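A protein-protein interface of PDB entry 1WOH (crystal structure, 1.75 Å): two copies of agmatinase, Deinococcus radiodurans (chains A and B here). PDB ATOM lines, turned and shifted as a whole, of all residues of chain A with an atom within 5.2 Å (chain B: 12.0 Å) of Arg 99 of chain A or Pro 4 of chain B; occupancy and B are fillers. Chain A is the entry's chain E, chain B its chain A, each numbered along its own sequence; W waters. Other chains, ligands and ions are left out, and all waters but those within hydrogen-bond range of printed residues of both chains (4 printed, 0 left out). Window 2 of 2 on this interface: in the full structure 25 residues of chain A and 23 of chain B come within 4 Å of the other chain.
His 6 of chain B touches Val 86 of chain A (CE1 to O, 3.4 Å). CD1 of Ile 87 of chain A touches O of Pro 4 of chain B (3.6 Å). Ala 5 of chain B touches Ile 87 of chain A. CG1 of Ile 87 of chain A touches NE2 of His 6 of chain B, 3.5 Å away. Leu 88 of chain A touches Leu 7 of chain B (O to CD2, 3.2 Å). NH2 of Arg 99 of chain A touches CB of Pro 4 of chain B, 3.8 Å away.
O of Leu 7 of chain B sits at hydrogen-bond distance from NH2 of Arg 17 of chain B (3.1 Å). O of Ile 87 of chain A lies within hydrogen-bond range of NH1 of Arg 99 of chain A (2.8 Å).
Of chain B, only His 6 comes within 4 Å of Val 86 of chain A. Of chain B, only Pro 4, Ala 5 and His 6 come within 4 Å of Ile 87 of chain A. Of chain B, only Leu 7 comes within 4 Å of Leu 88 of chain A. No residue of chain B comes within 4 Å of Pro 89 of chain A. No residue of chain B comes within 4 Å of Leu 95 of chain A. No residue of chain B comes within 4 Å of Ala 96 of chain A. His 97 of chain A touches none of the printed residues of chain B. No residue of chain B comes within 4 Å of Ile 100 of chain A. No residue of chain B comes within 4 Å of Thr 101 of chain A. Of the printed residues of chain A, Pro 4 of chain B touches Ile 87 and Arg 99. Printed residues of chain A within 4 Å of Ala 5 of chain B: Ile 87 (3.8 Å). Printed residues of chain A within 4 Å of His 6 of chain B: Val 86 and Ile 87. Printed residues of chain A within 4 Å of Leu 7 of chain B: Leu 88 (3.2 Å). Gly 11 of chain B touches none of the printed residues of chain A.
No position is printed for both chains. Of the 6 pairs that touch across the chains among the printed residues, none has its exchanged pair printed and touching as well.
Hydrophobic or aromatic side chains of chain B that line the printed part of chain A: Pro 4, His 6 and Leu 7.
Water W4 bridges the side-chain hydroxyl (OH) of Tyr 9 of chain B and the backbone carbonyl oxygen (O) of Pro 89 of chain A. Water W1 lies within hydrogen-bond range of the backbone carbonyl oxygen of Ala 5 of chain B and the backbone carbonyl oxygen of Leu 88 of chain A. Water W3 lies within hydrogen-bond range of the backbone carbonyl oxygen (O) of Val 86 of chain A (2.8 Å), a ring nitrogen (ND1) of His 6 of chain B (2.9 Å) and the backbone NH (N) of Leu 88 of chain A (3.0 Å). Water W2 bridges O of Leu 88 of chain A (2.9 Å) and N of Leu 7 of chain B (3.0 Å).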
ATOM      1  N   VAL A  86     -13.366   0.665 -21.930  1.00  0.00           N
ATOM      2  CA  VAL A  86     -13.665   0.270 -23.295  1.00  0.00           C
ATOM      3  C   VAL A  86     -12.295  -0.032 -23.897  1.00  0.00           C
ATOM      4  O   VAL A  86     -11.333   0.702 -23.657  1.00  0.00           O
ATOM      5  CB  VAL A  86     -14.321   1.429 -24.075  1.00  0.00           C
ATOM      6  CG1 VAL A  86     -14.473   1.058 -25.545  1.00  0.00           C
ATOM      7  CG2 VAL A  86     -15.679   1.762 -23.463  1.00  0.00           C
ATOM      8  N   ILE A  87     -12.185  -1.124 -24.647  1.00  0.00           N
ATOM      9  CA  ILE A  87     -10.912  -1.455 -25.276  1.00  0.00           C
ATOM     10  C   ILE A  87     -10.838  -0.597 -26.530  1.00  0.00           C
ATOM     11  O   ILE A  87     -11.525  -0.855 -27.519  1.00  0.00           O
ATOM     12  CB  ILE A  87     -10.831  -2.947 -25.649  1.00  0.00           C
ATOM     13  CG1 ILE A  87     -10.914  -3.801 -24.378  1.00  0.00           C
ATOM     14  CG2 ILE A  87      -9.524  -3.220 -26.382  1.00  0.00           C
ATOM     15  CD1 ILE A  87     -10.910  -5.303 -24.624  1.00  0.00           C
ATOM     16  N   LEU A  88     -10.009   0.436 -26.477  1.00  0.00           N
ATOM     17  CA  LEU A  88      -9.882   1.370 -27.585  1.00  0.00           C
ATOM     18  C   LEU A  88      -8.719   1.056 -28.501  1.00  0.00           C
ATOM     19  O   LEU A  88      -7.708   0.507 -28.076  1.00  0.00           O
ATOM     20  CB  LEU A  88      -9.701   2.795 -27.044  1.00  0.00           C
ATOM     21  CG  LEU A  88     -10.741   3.347 -26.063  1.00  0.00           C
ATOM     22  CD1 LEU A  88     -10.153   4.548 -25.338  1.00  0.00           C
ATOM     23  CD2 LEU A  88     -12.016   3.723 -26.797  1.00  0.00           C
ATOM     24  N   PRO A  89      -8.855   1.399 -29.790  1.00  0.00           N
ATOM     25  CA  PRO A  89      -7.784   1.154 -30.754  1.00  0.00           C
ATOM     26  C   PRO A  89      -6.899   2.398 -30.694  1.00  0.00           C
ATOM     27  O   PRO A  89      -7.223   3.348 -29.983  1.00  0.00           O
ATOM     28  CB  PRO A  89      -8.538   1.069 -32.072  1.00  0.00           C
ATOM     29  CG  PRO A  89      -9.579   2.149 -31.891  1.00  0.00           C
ATOM     30  CD  PRO A  89     -10.071   1.886 -30.471  1.00  0.00           C
ATOM     31  N   LEU A  95     -13.809   3.883 -35.121  1.00  0.00           N
ATOM     32  CA  LEU A  95     -13.890   2.561 -34.507  1.00  0.00           C
ATOM     33  C   LEU A  95     -14.022   2.730 -32.993  1.00  0.00           C
ATOM     34  O   LEU A  95     -14.815   2.044 -32.342  1.00  0.00           O
ATOM     35  CB  LEU A  95     -12.634   1.746 -34.830  1.00  0.00           C
ATOM     36  CG  LEU A  95     -12.468   0.404 -34.113  1.00  0.00           C
ATOM     37  CD1 LEU A  95     -13.647  -0.510 -34.425  1.00  0.00           C
ATOM     38  CD2 LEU A  95     -11.155  -0.235 -34.543  1.00  0.00           C
ATOM     39  N   ALA A  96     -13.247   3.655 -32.439  1.00  0.00           N
ATOM     40  CA  ALA A  96     -13.294   3.921 -31.005  1.00  0.00           C
ATOM     41  C   ALA A  96     -14.725   4.274 -30.623  1.00  0.00           C
ATOM     42  O   ALA A  96     -15.251   3.782 -29.630  1.00  0.00           O
ATOM     43  CB  ALA A  96     -12.352   5.072 -30.647  1.00  0.00           C
ATOM     44  N   HIS A  97     -15.347   5.128 -31.431  1.00  0.00           N
ATOM     45  CA  HIS A  97     -16.725   5.558 -31.201  1.00  0.00           C
ATOM     46  C   HIS A  97     -17.688   4.380 -31.114  1.00  0.00           C
ATOM     47  O   HIS A  97     -18.526   4.313 -30.214  1.00  0.00           O
ATOM     48  CB  HIS A  97     -17.176   6.496 -32.327  1.00  0.00           C
ATOM     49  CG  HIS A  97     -16.483   7.824 -32.324  1.00  0.00           C
ATOM     50  ND1 HIS A  97     -16.567   8.707 -33.380  1.00  0.00           N
ATOM     51  CD2 HIS A  97     -15.714   8.431 -31.388  1.00  0.00           C
ATOM     52  CE1 HIS A  97     -15.881   9.799 -33.095  1.00  0.00           C
ATOM     53  NE2 HIS A  97     -15.353   9.657 -31.892  1.00  0.00           N
ATOM     54  N   ASP A  98     -17.573   3.452 -32.057  1.00  0.00           N
ATOM     55  CA  ASP A  98     -18.438   2.288 -32.059  1.00  0.00           C
ATOM     56  C   ASP A  98     -18.172   1.409 -30.842  1.00  0.00           C
ATOM     57  O   ASP A  98     -19.108   0.892 -30.234  1.00  0.00           O
ATOM     58  CB  ASP A  98     -18.254   1.477 -33.348  1.00  0.00           C
ATOM     59  CG  ASP A  98     -18.751   2.218 -34.579  1.00  0.00           C
ATOM     60  OD1 ASP A  98     -19.585   3.138 -34.426  1.00  0.00           O
ATOM     61  OD2 ASP A  98     -18.319   1.871 -35.700  1.00  0.00           O
ATOM     62  N   ARG A  99     -16.898   1.249 -30.486  1.00  0.00           N
ATOM     63  CA  ARG A  99     -16.516   0.441 -29.329  1.00  0.00           C
ATOM     64  C   ARG A  99     -17.176   1.023 -28.081  1.00  0.00           C
ATOM     65  O   ARG A  99     -17.736   0.301 -27.251  1.00  0.00           O
ATOM     66  CB  ARG A  99     -14.991   0.459 -29.149  1.00  0.00           C
ATOM     67  CG  ARG A  99     -14.182  -0.213 -30.263  1.00  0.00           C
ATOM     68  CD  ARG A  99     -14.017  -1.707 -30.021  1.00  0.00           C
ATOM     69  NE  ARG A  99     -13.171  -2.354 -31.026  1.00  0.00           N
ATOM     70  CZ  ARG A  99     -11.842  -2.286 -31.069  1.00  0.00           C
ATOM     71  NH1 ARG A  99     -11.166  -1.594 -30.158  1.00  0.00           N
ATOM     72  NH2 ARG A  99     -11.180  -2.917 -32.032  1.00  0.00           N
ATOM     73  N   ILE A 100     -17.109   2.343 -27.966  1.00  0.00           N
ATOM     74  CA  ILE A 100     -17.671   3.057 -26.830  1.00  0.00           C
ATOM     75  C   ILE A 100     -19.189   2.931 -26.729  1.00  0.00           C
ATOM     76  O   ILE A 100     -19.730   2.643 -25.660  1.00  0.00           O
ATOM     77  CB  ILE A 100     -17.276   4.546 -26.895  1.00  0.00           C
ATOM     78  CG1 ILE A 100     -15.753   4.673 -26.783  1.00  0.00           C
ATOM     79  CG2 ILE A 100     -17.975   5.321 -25.793  1.00  0.00           C
ATOM     80  CD1 ILE A 100     -15.227   6.060 -27.081  1.00  0.00           C
ATOM     81  N   THR A 101     -19.875   3.132 -27.845  1.00  0.00           N
ATOM     82  CA  THR A 101     -21.328   3.028 -27.854  1.00  0.00           C
ATOM     83  C   THR A 101     -21.803   1.633 -27.450  1.00  0.00           C
ATOM     84  O   THR A 101     -22.695   1.490 -26.608  1.00  0.00           O
ATOM     85  CB  THR A 101     -21.898   3.359 -29.245  1.00  0.00           C
ATOM     86  OG1 THR A 101     -21.580   4.719 -29.580  1.00  0.00           O
ATOM     87  CG2 THR A 101     -23.423   3.174 -29.248  1.00  0.00           C
ATOM     88  N   GLU A 102     -21.208   0.603 -28.042  1.00  0.00           N
ATOM     89  CA  GLU A 102     -21.613  -0.761 -27.725  1.00  0.00           C
ATOM     90  C   GLU A 102     -21.378  -1.110 -26.262  1.00  0.00           C
ATOM     91  O   GLU A 102     -22.246  -1.693 -25.611  1.00  0.00           O
ATOM     92  CB  GLU A 102     -20.885  -1.768 -28.617  1.00  0.00           C
ATOM     93  CG  GLU A 102     -21.238  -3.220 -28.299  1.00  0.00           C
ATOM     94  CD  GLU A 102     -22.737  -3.504 -28.359  1.00  0.00           C
ATOM     95  OE1 GLU A 102     -23.145  -4.619 -27.965  1.00  0.00           O
ATOM     96  OE2 GLU A 102     -23.511  -2.626 -28.798  1.00  0.00           O
ATOM     97  N   ALA A 103     -20.205  -0.753 -25.748  1.00  0.00           N
ATOM     98  CA  ALA A 103     -19.876  -1.032 -24.356  1.00  0.00           C
ATOM     99  C   ALA A 103     -20.845  -0.285 -23.449  1.00  0.00           C
ATOM    100  O   ALA A 103     -21.324  -0.829 -22.452  1.00  0.00           O
ATOM    101  CB  ALA A 103     -18.435  -0.608 -24.058  1.00  0.00           C
ATOM    102  N   ALA A 104     -21.146   0.960 -23.809  1.00  0.00           N
ATOM    103  CA  ALA A 104     -22.057   1.772 -23.015  1.00  0.00           C
ATOM    104  C   ALA A 104     -23.461   1.168 -22.967  1.00  0.00           C
ATOM    105  O   ALA A 104     -24.117   1.210 -21.931  1.00  0.00           O
ATOM    106  CB  ALA A 104     -22.102   3.201 -23.564  1.00  0.00           C
ATOM    107  N   GLY B   3      -8.774 -11.209 -30.008  1.00  0.00           N
ATOM    108  CA  GLY B   3      -9.550  -9.943 -29.868  1.00  0.00           C
ATOM    109  C   GLY B   3      -8.670  -8.754 -29.523  1.00  0.00           C
ATOM    110  O   GLY B   3      -7.478  -8.924 -29.252  1.00  0.00           O
ATOM    111  N   PRO B   4      -9.227  -7.532 -29.521  1.00  0.00           N
ATOM    112  CA  PRO B   4      -8.456  -6.326 -29.202  1.00  0.00           C
ATOM    113  C   PRO B   4      -7.933  -6.331 -27.765  1.00  0.00           C
ATOM    114  O   PRO B   4      -8.596  -6.834 -26.855  1.00  0.00           O
ATOM    115  CB  PRO B   4      -9.456  -5.202 -29.460  1.00  0.00           C
ATOM    116  CG  PRO B   4     -10.762  -5.837 -29.097  1.00  0.00           C
ATOM    117  CD  PRO B   4     -10.647  -7.201 -29.744  1.00  0.00           C
ATOM    118  N   ALA B   5      -6.743  -5.771 -27.574  1.00  0.00           N
ATOM    119  CA  ALA B   5      -6.117  -5.710 -26.258  1.00  0.00           C
ATOM    120  C   ALA B   5      -5.924  -4.270 -25.796  1.00  0.00           C
ATOM    121  O   ALA B   5      -5.578  -3.393 -26.590  1.00  0.00           O
ATOM    122  CB  ALA B   5      -4.771  -6.430 -26.288  1.00  0.00           C
ATOM    123  N   HIS B   6      -6.152  -4.036 -24.506  1.00  0.00           N
ATOM    124  CA  HIS B   6      -5.997  -2.707 -23.921  1.00  0.00           C
ATOM    125  C   HIS B   6      -4.591  -2.166 -24.133  1.00  0.00           C
ATOM    126  O   HIS B   6      -3.634  -2.930 -24.277  1.00  0.00           O
ATOM    127  CB  HIS B   6      -6.258  -2.747 -22.407  1.00  0.00           C
ATOM    128  CG  HIS B   6      -7.704  -2.656 -22.027  1.00  0.00           C
ATOM    129  ND1 HIS B   6      -8.490  -1.569 -22.345  1.00  0.00           N
ATOM    130  CD2 HIS B   6      -8.499  -3.505 -21.334  1.00  0.00           C
ATOM    131  CE1 HIS B   6      -9.707  -1.753 -21.865  1.00  0.00           C
ATOM    132  NE2 HIS B   6      -9.739  -2.920 -21.247  1.00  0.00           N
ATOM    133  N   LEU B   7      -4.481  -0.842 -24.163  1.00  0.00           N
ATOM    134  CA  LEU B   7      -3.193  -0.177 -24.280  1.00  0.00           C
ATOM    135  C   LEU B   7      -2.751  -0.077 -22.822  1.00  0.00           C
ATOM    136  O   LEU B   7      -3.548  -0.330 -21.921  1.00  0.00           O
ATOM    137  CB  LEU B   7      -3.351   1.225 -24.875  1.00  0.00           C
ATOM    138  CG  LEU B   7      -3.570   1.365 -26.385  1.00  0.00           C
ATOM    139  CD1 LEU B   7      -2.312   0.957 -27.128  1.00  0.00           C
ATOM    140  CD2 LEU B   7      -4.748   0.518 -26.815  1.00  0.00           C
ATOM    141  N   PRO B   8      -1.486   0.289 -22.566  1.00  0.00           N
ATOM    142  CA  PRO B   8      -1.002   0.398 -21.183  1.00  0.00           C
ATOM    143  C   PRO B   8      -1.860   1.269 -20.258  1.00  0.00           C
ATOM    144  O   PRO B   8      -1.988   0.981 -19.068  1.00  0.00           O
ATOM    145  CB  PRO B   8       0.407   0.959 -21.357  1.00  0.00           C
ATOM    146  CG  PRO B   8       0.835   0.358 -22.657  1.00  0.00           C
ATOM    147  CD  PRO B   8      -0.394   0.545 -23.522  1.00  0.00           C
ATOM    148  N   TYR B   9      -2.448   2.329 -20.802  1.00  0.00           N
ATOM    149  CA  TYR B   9      -3.269   3.229 -19.996  1.00  0.00           C
ATOM    150  C   TYR B   9      -4.719   2.786 -19.830  1.00  0.00           C
ATOM    151  O   TYR B   9      -5.510   3.474 -19.184  1.00  0.00           O
ATOM    152  CB  TYR B   9      -3.241   4.639 -20.584  1.00  0.00           C
ATOM    153  CG  TYR B   9      -3.520   4.696 -22.068  1.00  0.00           C
ATOM    154  CD1 TYR B   9      -2.502   4.487 -22.995  1.00  0.00           C
ATOM    155  CD2 TYR B   9      -4.803   4.965 -22.548  1.00  0.00           C
ATOM    156  CE1 TYR B   9      -2.750   4.551 -24.363  1.00  0.00           C
ATOM    157  CE2 TYR B   9      -5.061   5.030 -23.917  1.00  0.00           C
ATOM    158  CZ  TYR B   9      -4.028   4.823 -24.816  1.00  0.00           C
ATOM    159  OH  TYR B   9      -4.268   4.901 -26.168  1.00  0.00           O
ATOM    160  N   GLY B  10      -5.074   1.642 -20.403  1.00  0.00           N
ATOM    161  CA  GLY B  10      -6.441   1.172 -20.282  1.00  0.00           C
ATOM    162  C   GLY B  10      -6.630  -0.057 -19.415  1.00  0.00           C
ATOM    163  O   GLY B  10      -5.730  -0.890 -19.286  1.00  0.00           O
ATOM    164  N   GLY B  11      -7.814  -0.164 -18.821  1.00  0.00           N
ATOM    165  CA  GLY B  11      -8.135  -1.306 -17.981  1.00  0.00           C
ATOM    166  C   GLY B  11      -7.767  -1.134 -16.520  1.00  0.00           C
ATOM    167  O   GLY B  11      -7.071  -0.187 -16.147  1.00  0.00           O
ATOM    168  N   ARG B  17      -1.678  -7.685 -15.721  1.00  0.00           N
ATOM    169  CA  ARG B  17      -3.063  -7.764 -16.182  1.00  0.00           C
ATOM    170  C   ARG B  17      -3.666  -9.136 -15.863  1.00  0.00           C
ATOM    171  O   ARG B  17      -4.541  -9.634 -16.571  1.00  0.00           O
ATOM    172  CB  ARG B  17      -3.138  -7.467 -17.688  1.00  0.00           C
ATOM    173  CG  ARG B  17      -4.378  -6.677 -18.098  1.00  0.00           C
ATOM    174  CD  ARG B  17      -4.449  -6.422 -19.604  1.00  0.00           C
ATOM    175  NE  ARG B  17      -3.793  -5.188 -20.049  1.00  0.00           N
ATOM    176  CZ  ARG B  17      -4.197  -3.963 -19.724  1.00  0.00           C
ATOM    177  NH1 ARG B  17      -5.250  -3.791 -18.935  1.00  0.00           N
ATOM    178  NH2 ARG B  17      -3.575  -2.902 -20.222  1.00  0.00           N
ATOM    179  N   VAL B  63       3.130  -7.103 -20.210  1.00  0.00           N
ATOM    180  CA  VAL B  63       2.210  -8.225 -20.080  1.00  0.00           C
ATOM    181  C   VAL B  63       2.763  -9.437 -20.833  1.00  0.00           C
ATOM    182  O   VAL B  63       3.084  -9.346 -22.018  1.00  0.00           O
ATOM    183  CB  VAL B  63       0.818  -7.869 -20.641  1.00  0.00           C
ATOM    184  CG1 VAL B  63      -0.136  -9.035 -20.447  1.00  0.00           C
ATOM    185  CG2 VAL B  63       0.283  -6.623 -19.947  1.00  0.00           C
HETATM  186  O   HOH W   1      -6.388  -1.902 -28.691  1.00  0.00           O
HETATM  187  O   HOH W   2      -7.128  -0.372 -25.405  1.00  0.00           O
HETATM  188  O   HOH W   3      -8.569   0.875 -23.825  1.00  0.00           O
HETATM  189  O   HOH W   4      -6.638   4.484 -27.182  1.00  0.00           O
